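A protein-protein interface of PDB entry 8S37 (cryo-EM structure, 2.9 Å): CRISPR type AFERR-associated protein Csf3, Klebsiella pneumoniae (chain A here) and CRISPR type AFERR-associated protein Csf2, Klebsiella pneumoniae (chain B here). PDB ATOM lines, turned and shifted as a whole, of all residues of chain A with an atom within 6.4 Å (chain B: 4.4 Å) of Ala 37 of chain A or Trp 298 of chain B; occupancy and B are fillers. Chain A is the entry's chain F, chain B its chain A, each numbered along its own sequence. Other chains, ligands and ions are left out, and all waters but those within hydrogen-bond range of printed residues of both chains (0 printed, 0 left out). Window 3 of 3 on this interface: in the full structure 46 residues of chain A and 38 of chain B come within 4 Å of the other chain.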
ATOM      1  N   GLU A  32       4.571 -12.592  12.430  1.00  0.00           N
ATOM      2  CA  GLU A  32       5.199 -13.427  13.449  1.00  0.00           C
ATOM      3  C   GLU A  32       4.436 -13.331  14.764  1.00  0.00           C
ATOM      4  O   GLU A  32       4.202 -14.343  15.440  1.00  0.00           O
ATOM      5  CB  GLU A  32       6.657 -13.016  13.639  1.00  0.00           C
ATOM      6  CG  GLU A  32       7.477 -13.986  14.475  1.00  0.00           C
ATOM      7  CD  GLU A  32       7.652 -15.335  13.806  1.00  0.00           C
ATOM      8  OE1 GLU A  32       7.510 -15.408  12.568  1.00  0.00           O
ATOM      9  OE2 GLU A  32       7.927 -16.322  14.520  1.00  0.00           O
ATOM     10  N   ALA A  33       4.031 -12.117  15.137  1.00  0.00           N
ATOM     11  CA  ALA A  33       3.291 -11.923  16.376  1.00  0.00           C
ATOM     12  C   ALA A  33       1.980 -12.693  16.358  1.00  0.00           C
ATOM     13  O   ALA A  33       1.568 -13.249  17.378  1.00  0.00           O
ATOM     14  CB  ALA A  33       3.034 -10.436  16.603  1.00  0.00           C
ATOM     15  N   LEU A  34       1.303 -12.730  15.209  1.00  0.00           N
ATOM     16  CA  LEU A  34       0.052 -13.473  15.114  1.00  0.00           C
ATOM     17  C   LEU A  34       0.305 -14.972  15.113  1.00  0.00           C
ATOM     18  O   LEU A  34      -0.414 -15.727  15.776  1.00  0.00           O
ATOM     19  CB  LEU A  34      -0.718 -13.065  13.862  1.00  0.00           C
ATOM     20  CG  LEU A  34      -1.755 -11.956  14.041  1.00  0.00           C
ATOM     21  CD1 LEU A  34      -2.305 -11.569  12.695  1.00  0.00           C
ATOM     22  CD2 LEU A  34      -2.886 -12.391  14.963  1.00  0.00           C
ATOM     23  N   SER A  35       1.321 -15.422  14.371  1.00  0.00           N
ATOM     24  CA  SER A  35       1.716 -16.824  14.412  1.00  0.00           C
ATOM     25  C   SER A  35       1.956 -17.276  15.840  1.00  0.00           C
ATOM     26  O   SER A  35       1.676 -18.428  16.186  1.00  0.00           O
ATOM     27  CB  SER A  35       2.974 -17.039  13.571  1.00  0.00           C
ATOM     28  OG  SER A  35       3.431 -18.374  13.680  1.00  0.00           O
ATOM     29  N   GLN A  36       2.473 -16.384  16.682  1.00  0.00           N
ATOM     30  CA  GLN A  36       2.578 -16.702  18.099  1.00  0.00           C
ATOM     31  C   GLN A  36       1.229 -16.595  18.802  1.00  0.00           C
ATOM     32  O   GLN A  36       0.921 -17.405  19.681  1.00  0.00           O
ATOM     33  CB  GLN A  36       3.578 -15.765  18.769  1.00  0.00           C
ATOM     34  CG  GLN A  36       5.015 -15.996  18.379  1.00  0.00           C
ATOM     35  CD  GLN A  36       5.943 -14.992  19.022  1.00  0.00           C
ATOM     36  OE1 GLN A  36       6.079 -14.948  20.243  1.00  0.00           O
ATOM     37  NE2 GLN A  36       6.577 -14.167  18.201  1.00  0.00           N
ATOM     38  N   ALA A  37       0.404 -15.617  18.422  1.00  0.00           N
ATOM     39  CA  ALA A  37      -0.831 -15.376  19.159  1.00  0.00           C
ATOM     40  C   ALA A  37      -1.887 -16.427  18.852  1.00  0.00           C
ATOM     41  O   ALA A  37      -2.559 -16.917  19.766  1.00  0.00           O
ATOM     42  CB  ALA A  37      -1.366 -13.981  18.840  1.00  0.00           C
ATOM     43  N   ILE A  38      -2.048 -16.785  17.582  1.00  0.00           N
ATOM     44  CA  ILE A  38      -2.784 -17.983  17.191  1.00  0.00           C
ATOM     45  C   ILE A  38      -1.756 -19.096  17.001  1.00  0.00           C
ATOM     46  O   ILE A  38      -0.935 -19.008  16.074  1.00  0.00           O
ATOM     47  CB  ILE A  38      -3.634 -17.769  15.929  1.00  0.00           C
ATOM     48  CG1 ILE A  38      -2.883 -17.016  14.825  1.00  0.00           C
ATOM     49  CG2 ILE A  38      -4.911 -17.015  16.282  1.00  0.00           C
ATOM     50  CD1 ILE A  38      -3.622 -16.978  13.509  1.00  0.00           C
ATOM     51  N   PRO A  39      -1.747 -20.137  17.835  1.00  0.00           N
ATOM     52  CA  PRO A  39      -0.612 -21.068  17.801  1.00  0.00           C
ATOM     53  C   PRO A  39      -0.631 -21.949  16.563  1.00  0.00           C
ATOM     54  O   PRO A  39      -0.794 -23.170  16.653  1.00  0.00           O
ATOM     55  CB  PRO A  39      -0.797 -21.876  19.088  1.00  0.00           C
ATOM     56  CG  PRO A  39      -2.267 -21.904  19.276  1.00  0.00           C
ATOM     57  CD  PRO A  39      -2.765 -20.566  18.811  1.00  0.00           C
ATOM     58  N   SER A  40      -0.475 -21.329  15.396  1.00  0.00           N
ATOM     59  CA  SER A  40      -0.508 -22.051  14.133  1.00  0.00           C
ATOM     60  C   SER A  40       0.397 -21.339  13.141  1.00  0.00           C
ATOM     61  O   SER A  40       0.328 -20.114  13.008  1.00  0.00           O
ATOM     62  CB  SER A  40      -1.938 -22.138  13.599  1.00  0.00           C
ATOM     63  OG  SER A  40      -2.171 -21.153  12.609  1.00  0.00           O
ATOM     64  N   ARG A  49      -5.932 -13.799   9.244  1.00  0.00           N
ATOM     65  CA  ARG A  49      -6.194 -13.096  10.492  1.00  0.00           C
ATOM     66  C   ARG A  49      -5.397 -11.804  10.609  1.00  0.00           C
ATOM     67  O   ARG A  49      -5.772 -10.929  11.397  1.00  0.00           O
ATOM     68  CB  ARG A  49      -5.870 -14.024  11.674  1.00  0.00           C
ATOM     69  CG  ARG A  49      -5.692 -13.365  13.050  1.00  0.00           C
ATOM     70  CD  ARG A  49      -6.949 -12.669  13.543  1.00  0.00           C
ATOM     71  NE  ARG A  49      -7.855 -13.602  14.201  1.00  0.00           N
ATOM     72  CZ  ARG A  49      -7.710 -14.047  15.442  1.00  0.00           C
ATOM     73  NH1 ARG A  49      -6.689 -13.677  16.200  1.00  0.00           N
ATOM     74  NH2 ARG A  49      -8.612 -14.891  15.937  1.00  0.00           N
ATOM     75  N   ILE A 146      -1.132  -4.479  21.213  1.00  0.00           N
ATOM     76  CA  ILE A 146      -1.070  -5.656  22.075  1.00  0.00           C
ATOM     77  C   ILE A 146      -0.014  -6.624  21.563  1.00  0.00           C
ATOM     78  O   ILE A 146       0.798  -7.152  22.335  1.00  0.00           O
ATOM     79  CB  ILE A 146      -2.452  -6.329  22.164  1.00  0.00           C
ATOM     80  CG1 ILE A 146      -3.435  -5.437  22.926  1.00  0.00           C
ATOM     81  CG2 ILE A 146      -2.337  -7.684  22.842  1.00  0.00           C
ATOM     82  CD1 ILE A 146      -4.892  -5.767  22.658  1.00  0.00           C
ATOM     83  N   LEU A 147       0.002  -6.858  20.252  1.00  0.00           N
ATOM     84  CA  LEU A 147       0.953  -7.798  19.672  1.00  0.00           C
ATOM     85  C   LEU A 147       2.384  -7.330  19.890  1.00  0.00           C
ATOM     86  O   LEU A 147       3.219  -8.072  20.418  1.00  0.00           O
ATOM     87  CB  LEU A 147       0.657  -7.971  18.183  1.00  0.00           C
ATOM     88  CG  LEU A 147      -0.629  -8.736  17.858  1.00  0.00           C
ATOM     89  CD1 LEU A 147      -0.971  -8.612  16.387  1.00  0.00           C
ATOM     90  CD2 LEU A 147      -0.506 -10.199  18.246  1.00  0.00           C
ATOM     91  N   HIS A 150       3.379  -7.549  23.653  1.00  0.00           N
ATOM     92  CA  HIS A 150       3.382  -8.832  24.344  1.00  0.00           C
ATOM     93  C   HIS A 150       3.822 -10.005  23.488  1.00  0.00           C
ATOM     94  O   HIS A 150       4.342 -10.978  24.037  1.00  0.00           O
ATOM     95  CB  HIS A 150       1.988  -9.121  24.906  1.00  0.00           C
ATOM     96  CG  HIS A 150       1.503  -8.069  25.850  1.00  0.00           C
ATOM     97  ND1 HIS A 150       2.194  -7.723  26.989  1.00  0.00           N
ATOM     98  CD2 HIS A 150       0.409  -7.274  25.815  1.00  0.00           C
ATOM     99  CE1 HIS A 150       1.542  -6.763  27.622  1.00  0.00           C
ATOM    100  NE2 HIS A 150       0.455  -6.473  26.931  1.00  0.00           N
ATOM    101  N   ALA A 151       3.646  -9.956  22.172  1.00  0.00           N
ATOM    102  CA  ALA A 151       4.218 -11.009  21.350  1.00  0.00           C
ATOM    103  C   ALA A 151       5.732 -10.862  21.319  1.00  0.00           C
ATOM    104  O   ALA A 151       6.272  -9.754  21.359  1.00  0.00           O
ATOM    105  CB  ALA A 151       3.654 -10.961  19.932  1.00  0.00           C
ATOM    106  N   HIS A 152       6.420 -11.997  21.246  1.00  0.00           N
ATOM    107  CA  HIS A 152       7.882 -12.007  21.272  1.00  0.00           C
ATOM    108  C   HIS A 152       8.418 -11.784  19.859  1.00  0.00           C
ATOM    109  O   HIS A 152       8.930 -12.685  19.195  1.00  0.00           O
ATOM    110  CB  HIS A 152       8.389 -13.308  21.871  1.00  0.00           C
ATOM    111  CG  HIS A 152       9.854 -13.301  22.163  1.00  0.00           C
ATOM    112  ND1 HIS A 152      10.402 -12.557  23.186  1.00  0.00           N
ATOM    113  CD2 HIS A 152      10.886 -13.942  21.568  1.00  0.00           C
ATOM    114  CE1 HIS A 152      11.710 -12.742  23.208  1.00  0.00           C
ATOM    115  NE2 HIS A 152      12.029 -13.577  22.236  1.00  0.00           N
ATOM    116  N   THR B   3       1.595 -20.696  22.711  1.00  0.00           N
ATOM    117  CA  THR B   3       2.770 -19.832  22.718  1.00  0.00           C
ATOM    118  C   THR B   3       2.928 -19.269  24.124  1.00  0.00           C
ATOM    119  O   THR B   3       2.092 -18.483  24.582  1.00  0.00           O
ATOM    120  CB  THR B   3       2.618 -18.716  21.688  1.00  0.00           C
ATOM    121  OG1 THR B   3       2.429 -19.287  20.389  1.00  0.00           O
ATOM    122  CG2 THR B   3       3.843 -17.806  21.662  1.00  0.00           C
ATOM    123  N   ASN B   5       4.767 -16.996  26.695  1.00  0.00           N
ATOM    124  CA  ASN B   5       5.609 -15.822  26.869  1.00  0.00           C
ATOM    125  C   ASN B   5       5.969 -15.709  28.345  1.00  0.00           C
ATOM    126  O   ASN B   5       5.103 -15.467  29.189  1.00  0.00           O
ATOM    127  CB  ASN B   5       4.895 -14.563  26.384  1.00  0.00           C
ATOM    128  CG  ASN B   5       4.240 -14.751  25.033  1.00  0.00           C
ATOM    129  OD1 ASN B   5       3.035 -14.977  24.943  1.00  0.00           O
ATOM    130  ND2 ASN B   5       5.032 -14.663  23.975  1.00  0.00           N
ATOM    131  N   THR B 297       0.148 -16.959  28.369  1.00  0.00           N
ATOM    132  CA  THR B 297      -0.153 -17.570  27.084  1.00  0.00           C
ATOM    133  C   THR B 297      -1.232 -16.739  26.410  1.00  0.00           C
ATOM    134  O   THR B 297      -1.808 -15.837  27.015  1.00  0.00           O
ATOM    135  CB  THR B 297      -0.618 -19.023  27.233  1.00  0.00           C
ATOM    136  OG1 THR B 297      -0.652 -19.649  25.946  1.00  0.00           O
ATOM    137  CG2 THR B 297      -2.011 -19.077  27.850  1.00  0.00           C
ATOM    138  N   TRP B 298      -1.505 -17.039  25.147  1.00  0.00           N
ATOM    139  CA  TRP B 298      -2.532 -16.335  24.391  1.00  0.00           C
ATOM    140  C   TRP B 298      -3.827 -17.133  24.415  1.00  0.00           C
ATOM    141  O   TRP B 298      -3.817 -18.347  24.189  1.00  0.00           O
ATOM    142  CB  TRP B 298      -2.082 -16.104  22.951  1.00  0.00           C
ATOM    143  CG  TRP B 298      -0.973 -15.115  22.837  1.00  0.00           C
ATOM    144  CD1 TRP B 298       0.362 -15.380  22.830  1.00  0.00           C
ATOM    145  CD2 TRP B 298      -1.103 -13.697  22.707  1.00  0.00           C
ATOM    146  NE1 TRP B 298       1.075 -14.214  22.706  1.00  0.00           N
ATOM    147  CE2 TRP B 298       0.197 -13.166  22.628  1.00  0.00           C
ATOM    148  CE3 TRP B 298      -2.192 -12.825  22.651  1.00  0.00           C
ATOM    149  CZ2 TRP B 298       0.438 -11.803  22.497  1.00  0.00           C
ATOM    150  CZ3 TRP B 298      -1.952 -11.473  22.520  1.00  0.00           C
ATOM    151  CH2 TRP B 298      -0.647 -10.975  22.445  1.00  0.00           C
ATOM    152  N   LYS B 299      -4.932 -16.451  24.701  1.00  0.00           N
ATOM    153  CA  LYS B 299      -6.237 -17.084  24.602  1.00  0.00           C
ATOM    154  C   LYS B 299      -6.441 -17.620  23.188  1.00  0.00           C
ATOM    155  O   LYS B 299      -6.042 -16.962  22.219  1.00  0.00           O
ATOM    156  CB  LYS B 299      -7.352 -16.097  24.941  1.00  0.00           C
ATOM    157  CG  LYS B 299      -7.577 -15.898  26.426  1.00  0.00           C
ATOM    158  CD  LYS B 299      -8.959 -15.325  26.722  1.00  0.00           C
ATOM    159  CE  LYS B 299     -10.056 -16.384  26.645  1.00  0.00           C
ATOM    160  NZ  LYS B 299      -9.922 -17.430  27.698  1.00  0.00           N
ATOM    161  N   PRO B 300      -7.028 -18.822  23.021  1.00  0.00           N
ATOM    162  CA  PRO B 300      -7.338 -19.289  21.663  1.00  0.00           C
ATOM    163  C   PRO B 300      -8.153 -18.273  20.880  1.00  0.00           C
ATOM    164  O   PRO B 300      -9.283 -17.944  21.252  1.00  0.00           O
ATOM    165  CB  PRO B 300      -8.131 -20.578  21.903  1.00  0.00           C
ATOM    166  CG  PRO B 300      -7.681 -21.055  23.225  1.00  0.00           C
ATOM    167  CD  PRO B 300      -7.404 -19.826  24.035  1.00  0.00           C
ATOM    168  N   GLU B 302      -8.552 -15.104  20.663  1.00  0.00           N
ATOM    169  CA  GLU B 302      -8.519 -13.740  21.167  1.00  0.00           C
ATOM    170  C   GLU B 302      -7.082 -13.259  21.342  1.00  0.00           C
ATOM    171  O   GLU B 302      -6.178 -14.028  21.679  1.00  0.00           O
ATOM    172  CB  GLU B 302      -9.269 -13.651  22.498  1.00  0.00           C
ATOM    173  CG  GLU B 302      -9.292 -12.264  23.134  1.00  0.00           C
ATOM    174  CD  GLU B 302      -9.880 -11.206  22.222  1.00  0.00           C
ATOM    175  OE1 GLU B 302     -10.677 -11.565  21.329  1.00  0.00           O
ATOM    176  OE2 GLU B 302      -9.544 -10.017  22.394  1.00  0.00           O
ATOM    177  N   LEU B 303      -6.883 -11.962  21.108  1.00  0.00           N
ATOM    178  CA  LEU B 303      -5.607 -11.296  21.372  1.00  0.00           C
ATOM    179  C   LEU B 303      -5.582 -10.752  22.802  1.00  0.00           C
ATOM    180  O   LEU B 303      -5.718  -9.553  23.048  1.00  0.00           O
ATOM    181  CB  LEU B 303      -5.373 -10.187  20.354  1.00  0.00           C
ATOM    182  CG  LEU B 303      -5.283 -10.635  18.896  1.00  0.00           C
ATOM    183  CD1 LEU B 303      -5.321  -9.432  17.972  1.00  0.00           C
ATOM    184  CD2 LEU B 303      -4.021 -11.449  18.663  1.00  0.00           C
ATOM    185  N   VAL B 304      -5.413 -11.661  23.758  1.00  0.00           N
ATOM    186  CA  VAL B 304      -5.282 -11.252  25.156  1.00  0.00           C
ATOM    187  C   VAL B 304      -4.388 -12.244  25.894  1.00  0.00           C
ATOM    188  O   VAL B 304      -4.507 -13.456  25.669  1.00  0.00           O
ATOM    189  CB  VAL B 304      -6.657 -11.137  25.832  1.00  0.00           C
ATOM    190  CG1 VAL B 304      -7.309 -12.502  25.977  1.00  0.00           C
ATOM    191  CG2 VAL B 304      -6.526 -10.455  27.187  1.00  0.00           C
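OG1 of Thr 3 of chain B lies within hydrogen-bond range of O of Gln 36 of chain A.
NE2 of Gln 36 of chain A is in hydrogen-bond range of O of His 152 of chain A (3.0 Å).
OD1 of Asn 5 of chain B lies within hydrogen-bond range of NE1 of Trp 298 of chain B, 3.1 Å away.
OG1 of Thr 297 of chain B is in hydrogen-bond range of O of Thr 3 of chain B, at 3.3 Å.
Among the printed residues, pairs that only touch across the chains: Leu 34 of chain A with Leu 303 of chain B, Gln 36 of chain A with Asn 5 of chain B, Gln 36 of chain A with Trp 298 of chain B, Ala 37 of chain A with Trp 298 of chain B, Ala 37 of chain A with Leu 303 of chain B, Ile 146 of chain A with Trp 298 of chain B, Ile 146 of chain A with Leu 303 of chain B, Leu 147 of chain A with Leu 303 of chain B, His 150 of chain A with Asn 5 of chain B, His 150 of chain A with Trp 298 of chain B and Ala 151 of chain A with Trp 298 of chain B.
Printed residues of chain B within 4 Å of Leu 34 of chain A: Leu 303 (3.98 Å).
Printed residues of chain B within 4 Å of Gln 36 of chain A: Thr 3, Asn 5 and Trp 298.
Ala 37 of chain A touches two residues of chain B.
Pro 39 of chain A touches none of the printed residues of chain B.
Printed residues of chain B within 4 Å of His 150 of chain A: Asn 5 and Trp 298.
Glu 302 of chain B touches none of the printed residues of chain A.
Printed residues of chain A within 4 Å of Leu 303 of chain B: Leu 34, Ala 37, Ile 146 and Leu 147.
Of the 15 printed residues of chain A, 7 touch a printed residue of chain B.
Hydrophobic or aromatic side chains of chain A within 4 Å of the printed part of chain B: Leu 34, Ala 37, Ile 146, Leu 147 and His 150.
Of the 9 printed residues of chain B, 4 touch a printed residue of chain A.
Hydrophobic or aromatic side chains of chain B that line the printed part of chain A: Trp 298 and Leu 303.
Among the printed residues, 12 pairs touch across the chains.
Among the printed residues, no Asp or Glu carboxylate lies within 4 Å of a Lys or Arg side-chain nitrogen of the other chain.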
